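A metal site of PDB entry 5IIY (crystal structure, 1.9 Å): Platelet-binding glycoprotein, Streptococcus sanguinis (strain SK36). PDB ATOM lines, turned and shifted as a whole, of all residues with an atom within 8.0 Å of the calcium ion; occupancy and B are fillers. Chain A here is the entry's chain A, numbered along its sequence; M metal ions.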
ATOM      1  N   ARG A   2      36.783 -22.208 -22.518  1.00  0.00           N
ATOM      2  CA  ARG A   2      36.774 -21.134 -21.532  1.00  0.00           C
ATOM      3  C   ARG A   2      37.579 -21.469 -20.277  1.00  0.00           C
ATOM      4  O   ARG A   2      37.320 -22.475 -19.617  1.00  0.00           O
ATOM      5  CB  ARG A   2      35.322 -20.789 -21.185  1.00  0.00           C
ATOM      6  CG  ARG A   2      35.107 -19.668 -20.185  1.00  0.00           C
ATOM      7  CD  ARG A   2      33.603 -19.413 -19.961  1.00  0.00           C
ATOM      8  NE  ARG A   2      32.857 -20.637 -19.676  1.00  0.00           N
ATOM      9  CZ  ARG A   2      32.158 -21.323 -20.589  1.00  0.00           C
ATOM     10  NH1 ARG A   2      32.098 -20.894 -21.846  1.00  0.00           N
ATOM     11  NH2 ARG A   2      31.519 -22.430 -20.241  1.00  0.00           N
ATOM     12  N   THR A   4      37.778 -20.100 -17.303  1.00  0.00           N
ATOM     13  CA  THR A   4      37.113 -20.013 -16.006  1.00  0.00           C
ATOM     14  C   THR A   4      35.592 -19.920 -16.138  1.00  0.00           C
ATOM     15  O   THR A   4      35.063 -19.473 -17.146  1.00  0.00           O
ATOM     16  CB  THR A   4      37.606 -18.783 -15.209  1.00  0.00           C
ATOM     17  OG1 THR A   4      37.427 -17.596 -15.999  1.00  0.00           O
ATOM     18  CG2 THR A   4      39.073 -18.928 -14.834  1.00  0.00           C
ATOM     19  N   ASP A   5      34.911 -20.364 -15.095  1.00  0.00           N
ATOM     20  CA  ASP A   5      33.461 -20.215 -14.973  1.00  0.00           C
ATOM     21  C   ASP A   5      33.153 -18.781 -14.540  1.00  0.00           C
ATOM     22  O   ASP A   5      33.541 -18.364 -13.449  1.00  0.00           O
ATOM     23  CB  ASP A   5      32.916 -21.224 -13.951  1.00  0.00           C
ATOM     24  CG  ASP A   5      31.379 -21.245 -13.861  1.00  0.00           C
ATOM     25  OD1 ASP A   5      30.696 -20.300 -14.315  1.00  0.00           O
ATOM     26  OD2 ASP A   5      30.838 -22.225 -13.302  1.00  0.00           O
ATOM     27  N   THR A   6      32.477 -18.024 -15.385  1.00  0.00           N
ATOM     28  CA  THR A   6      32.130 -16.642 -15.054  1.00  0.00           C
ATOM     29  C   THR A   6      30.626 -16.414 -15.137  1.00  0.00           C
ATOM     30  O   THR A   6      30.154 -15.284 -15.066  1.00  0.00           O
ATOM     31  CB  THR A   6      32.832 -15.640 -15.979  1.00  0.00           C
ATOM     32  OG1 THR A   6      32.465 -15.915 -17.334  1.00  0.00           O
ATOM     33  CG2 THR A   6      34.346 -15.741 -15.830  1.00  0.00           C
ATOM     34  N   THR A   7      29.882 -17.506 -15.275  1.00  0.00           N
ATOM     35  CA  THR A   7      28.436 -17.435 -15.468  1.00  0.00           C
ATOM     36  C   THR A   7      27.697 -17.912 -14.232  1.00  0.00           C
ATOM     37  O   THR A   7      27.940 -19.006 -13.768  1.00  0.00           O
ATOM     38  CB  THR A   7      28.032 -18.289 -16.684  1.00  0.00           C
ATOM     39  OG1 THR A   7      28.826 -17.908 -17.814  1.00  0.00           O
ATOM     40  CG2 THR A   7      26.556 -18.102 -17.000  1.00  0.00           C
ATOM     41  N   PRO A   8      26.778 -17.099 -13.687  1.00  0.00           N
ATOM     42  CA  PRO A   8      26.080 -17.554 -12.473  1.00  0.00           C
ATOM     43  C   PRO A   8      24.998 -18.595 -12.792  1.00  0.00           C
ATOM     44  O   PRO A   8      24.648 -18.790 -13.950  1.00  0.00           O
ATOM     45  CB  PRO A   8      25.467 -16.257 -11.931  1.00  0.00           C
ATOM     46  CG  PRO A   8      25.267 -15.402 -13.135  1.00  0.00           C
ATOM     47  CD  PRO A   8      26.372 -15.745 -14.093  1.00  0.00           C
ATOM     48  N   PRO A   9      24.473 -19.267 -11.751  1.00  0.00           N
ATOM     49  CA  PRO A   9      23.375 -20.201 -11.929  1.00  0.00           C
ATOM     50  C   PRO A   9      22.128 -19.559 -12.513  1.00  0.00           C
ATOM     51  O   PRO A   9      21.956 -18.340 -12.447  1.00  0.00           O
ATOM     52  CB  PRO A   9      23.089 -20.697 -10.504  1.00  0.00           C
ATOM     53  CG  PRO A   9      24.366 -20.518  -9.783  1.00  0.00           C
ATOM     54  CD  PRO A   9      25.018 -19.300 -10.376  1.00  0.00           C
ATOM     55  N   THR A  10      21.257 -20.398 -13.061  1.00  0.00           N
ATOM     56  CA  THR A  10      19.983 -19.975 -13.641  1.00  0.00           C
ATOM     57  C   THR A  10      18.851 -20.588 -12.828  1.00  0.00           C
ATOM     58  O   THR A  10      18.807 -21.794 -12.671  1.00  0.00           O
ATOM     59  CB  THR A  10      19.857 -20.425 -15.117  1.00  0.00           C
ATOM     60  OG1 THR A  10      20.874 -19.803 -15.900  1.00  0.00           O
ATOM     61  CG2 THR A  10      18.505 -20.037 -15.683  1.00  0.00           C
ATOM     62  N   THR A  32      20.006 -24.599 -12.418  1.00  0.00           N
ATOM     63  CA  THR A  32      21.069 -25.199 -13.212  1.00  0.00           C
ATOM     64  C   THR A  32      22.275 -24.249 -13.250  1.00  0.00           C
ATOM     65  O   THR A  32      22.123 -23.052 -13.060  1.00  0.00           O
ATOM     66  CB  THR A  32      20.621 -25.479 -14.666  1.00  0.00           C
ATOM     67  OG1 THR A  32      20.403 -24.240 -15.346  1.00  0.00           O
ATOM     68  CG2 THR A  32      19.338 -26.302 -14.707  1.00  0.00           C
ATOM     69  N   ASP A  33      23.472 -24.801 -13.487  1.00  0.00           N
ATOM     70  CA  ASP A  33      24.652 -23.963 -13.727  1.00  0.00           C
ATOM     71  C   ASP A  33      25.494 -24.613 -14.801  1.00  0.00           C
ATOM     72  O   ASP A  33      25.523 -25.843 -14.912  1.00  0.00           O
ATOM     73  CB  ASP A  33      25.470 -23.758 -12.454  1.00  0.00           C
ATOM     74  CG  ASP A  33      26.661 -22.823 -12.663  1.00  0.00           C
ATOM     75  OD1 ASP A  33      26.464 -21.599 -12.706  1.00  0.00           O
ATOM     76  OD2 ASP A  33      27.806 -23.307 -12.778  1.00  0.00           O
ATOM     77  N   ASP A  34      26.181 -23.797 -15.601  1.00  0.00           N
ATOM     78  CA  ASP A  34      26.966 -24.332 -16.717  1.00  0.00           C
ATOM     79  C   ASP A  34      28.035 -25.326 -16.248  1.00  0.00           C
ATOM     80  O   ASP A  34      28.434 -26.215 -16.975  1.00  0.00           O
ATOM     81  CB  ASP A  34      27.599 -23.195 -17.532  1.00  0.00           C
ATOM     82  CG  ASP A  34      28.515 -22.289 -16.715  1.00  0.00           C
ATOM     83  OD1 ASP A  34      28.272 -22.096 -15.497  1.00  0.00           O
ATOM     84  OD2 ASP A  34      29.488 -21.750 -17.286  1.00  0.00           O
ATOM     85  N   SER A  35      28.465 -25.179 -14.990  1.00  0.00           N
ATOM     86  CA  SER A  35      29.403 -26.098 -14.354  1.00  0.00           C
ATOM     87  C   SER A  35      28.757 -27.403 -13.874  1.00  0.00           C
ATOM     88  O   SER A  35      29.465 -28.383 -13.583  1.00  0.00           O
ATOM     89  CB  SER A  35      30.062 -25.437 -13.148  1.00  0.00           C
ATOM     90  OG  SER A  35      29.175 -25.424 -12.040  1.00  0.00           O
ATOM     91  N   GLY A  36      27.442 -27.401 -13.752  1.00  0.00           N
ATOM     92  CA  GLY A  36      26.733 -28.544 -13.205  1.00  0.00           C
ATOM     93  C   GLY A  36      26.677 -28.589 -11.687  1.00  0.00           C
ATOM     94  O   GLY A  36      26.102 -29.521 -11.121  1.00  0.00           O
ATOM     95  N   GLN A  37      27.273 -27.613 -11.012  1.00  0.00           N
ATOM     96  CA  GLN A  37      27.260 -27.588  -9.553  1.00  0.00           C
ATOM     97  C   GLN A  37      26.774 -26.268  -8.979  1.00  0.00           C
ATOM     98  O   GLN A  37      27.303 -25.198  -9.290  1.00  0.00           O
ATOM     99  CB  GLN A  37      28.654 -27.899  -9.010  1.00  0.00           C
ATOM    100  CG  GLN A  37      28.720 -27.967  -7.480  1.00  0.00           C
ATOM    101  CD  GLN A  37      30.075 -28.415  -6.983  1.00  0.00           C
ATOM    102  OE1 GLN A  37      30.881 -28.940  -7.736  1.00  0.00           O
ATOM    103  NE2 GLN A  37      30.346 -28.181  -5.690  1.00  0.00           N
ATOM    104  N   VAL A  38      25.761 -26.339  -8.120  1.00  0.00           N
ATOM    105  CA  VAL A  38      25.268 -25.174  -7.384  1.00  0.00           C
ATOM    106  C   VAL A  38      25.638 -25.328  -5.906  1.00  0.00           C
ATOM    107  O   VAL A  38      25.402 -26.392  -5.317  1.00  0.00           O
ATOM    108  CB  VAL A  38      23.754 -24.999  -7.560  1.00  0.00           C
ATOM    109  CG1 VAL A  38      23.165 -24.090  -6.472  1.00  0.00           C
ATOM    110  CG2 VAL A  38      23.445 -24.453  -8.949  1.00  0.00           C
ATOM    111  N   TRP A 104      24.477 -19.351  -5.751  1.00  0.00           N
ATOM    112  CA  TRP A 104      25.904 -19.375  -6.046  1.00  0.00           C
ATOM    113  C   TRP A 104      26.288 -20.671  -6.749  1.00  0.00           C
ATOM    114  O   TRP A 104      25.748 -21.731  -6.438  1.00  0.00           O
ATOM    115  CB  TRP A 104      26.722 -19.275  -4.748  1.00  0.00           C
ATOM    116  CG  TRP A 104      26.810 -17.934  -4.085  1.00  0.00           C
ATOM    117  CD1 TRP A 104      27.869 -17.072  -4.131  1.00  0.00           C
ATOM    118  CD2 TRP A 104      25.826 -17.320  -3.246  1.00  0.00           C
ATOM    119  NE1 TRP A 104      27.599 -15.946  -3.399  1.00  0.00           N
ATOM    120  CE2 TRP A 104      26.352 -16.073  -2.840  1.00  0.00           C
ATOM    121  CE3 TRP A 104      24.553 -17.695  -2.808  1.00  0.00           C
ATOM    122  CZ2 TRP A 104      25.655 -15.196  -2.020  1.00  0.00           C
ATOM    123  CZ3 TRP A 104      23.847 -16.819  -1.991  1.00  0.00           C
ATOM    124  CH2 TRP A 104      24.400 -15.583  -1.602  1.00  0.00           C
ATOM    125  N   ASP A 105      27.240 -20.603  -7.676  1.00  0.00           N
ATOM    126  CA  ASP A 105      27.872 -21.838  -8.119  1.00  0.00           C
ATOM    127  C   ASP A 105      29.112 -22.058  -7.253  1.00  0.00           C
ATOM    128  O   ASP A 105      29.286 -21.382  -6.236  1.00  0.00           O
ATOM    129  CB  ASP A 105      28.207 -21.823  -9.617  1.00  0.00           C
ATOM    130  CG  ASP A 105      29.181 -20.715 -10.015  1.00  0.00           C
ATOM    131  OD1 ASP A 105      29.870 -20.143  -9.141  1.00  0.00           O
ATOM    132  OD2 ASP A 105      29.261 -20.437 -11.226  1.00  0.00           O
ATOM    133  N   ALA A 106      29.961 -23.002  -7.636  1.00  0.00           N
ATOM    134  CA  ALA A 106      31.135 -23.305  -6.828  1.00  0.00           C
ATOM    135  C   ALA A 106      32.346 -22.473  -7.218  1.00  0.00           C
ATOM    136  O   ALA A 106      33.442 -22.681  -6.694  1.00  0.00           O
ATOM    137  CB  ALA A 106      31.475 -24.792  -6.931  1.00  0.00           C
ATOM    138  N   ALA A 107      32.143 -21.521  -8.134  1.00  0.00           N
ATOM    139  CA  ALA A 107      33.234 -20.672  -8.605  1.00  0.00           C
ATOM    140  C   ALA A 107      33.083 -19.213  -8.162  1.00  0.00           C
ATOM    141  O   ALA A 107      33.781 -18.335  -8.660  1.00  0.00           O
ATOM    142  CB  ALA A 107      33.341 -20.751 -10.121  1.00  0.00           C
ATOM    143  N   GLY A 108      32.145 -18.960  -7.260  1.00  0.00           N
ATOM    144  CA  GLY A 108      31.957 -17.626  -6.721  1.00  0.00           C
ATOM    145  C   GLY A 108      30.964 -16.746  -7.471  1.00  0.00           C
ATOM    146  O   GLY A 108      30.752 -15.595  -7.083  1.00  0.00           O
ATOM    147  N   ASN A 109      30.363 -17.272  -8.534  1.00  0.00           N
ATOM    148  CA  ASN A 109      29.353 -16.525  -9.275  1.00  0.00           C
ATOM    149  C   ASN A 109      27.984 -16.650  -8.611  1.00  0.00           C
ATOM    150  O   ASN A 109      27.484 -17.750  -8.416  1.00  0.00           O
ATOM    151  CB  ASN A 109      29.256 -17.019 -10.713  1.00  0.00           C
ATOM    152  CG  ASN A 109      30.601 -17.034 -11.409  1.00  0.00           C
ATOM    153  OD1 ASN A 109      31.207 -15.987 -11.633  1.00  0.00           O
ATOM    154  ND2 ASN A 109      31.067 -18.222 -11.766  1.00  0.00           N
ATOM    155  N   VAL A 110      27.387 -15.501  -8.305  1.00  0.00           N
ATOM    156  CA  VAL A 110      26.048 -15.478  -7.718  1.00  0.00           C
ATOM    157  C   VAL A 110      25.073 -14.828  -8.713  1.00  0.00           C
ATOM    158  O   VAL A 110      25.394 -13.837  -9.369  1.00  0.00           O
ATOM    159  CB  VAL A 110      26.031 -14.721  -6.362  1.00  0.00           C
ATOM    160  CG1 VAL A 110      26.442 -13.268  -6.527  1.00  0.00           C
ATOM    161  CG2 VAL A 110      24.655 -14.811  -5.709  1.00  0.00           C
HETATM  162 CA    CA M   1      28.706 -21.206 -13.370  1.00  0.00          CA
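The side-chain carboxylate of Asp 33 sits close to the side-chain hydroxyl of Ser 35 (2.6 Å). The backbone carbonyl oxygen of Asp 5 is in hydrogen-bond range of the side-chain amide nitrogen of Asn 109 (3.0 Å). The side-chain carboxylate (OD1) of Asp 105 lies within hydrogen-bond range of the backbone NH (N) of Gly 108, 3.2 Å away. The side-chain carboxylate (OD2) of Asp 34 is in salt-bridge range of the guanidinium group (NH2) of Arg 2 (3.6 Å). The backbone NH of Asn 109 sits at hydrogen-bond distance from the side-chain carboxylate of Asp 105 (3.0 Å). The side-chain carboxylate (OD1) of Asp 105 lies within hydrogen-bond range of the backbone NH (N) of Ala 107.
Of the 22 residues printed, 5 come within 4 Å of the calcium ion. The nearest printed residue that does not touch the calcium ion is Asn 109 (4.1 Å).
OD2 of Asp 105 binds the calcium ion. The calcium ion is bound by OD1 of Asp 34, at 2.3 Å. OD2 of Asp 33 is bound to the calcium ion (2.4 Å). O of Thr 7 binds the calcium ion (2.4 Å). The side-chain carboxylate (OD2) of Asp 5 is bound to the calcium ion. The side-chain carboxylate (OD1) of Asp 33 binds the calcium ion (2.4 Å). OD1 of Asp 5 is bound to the calcium ion.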
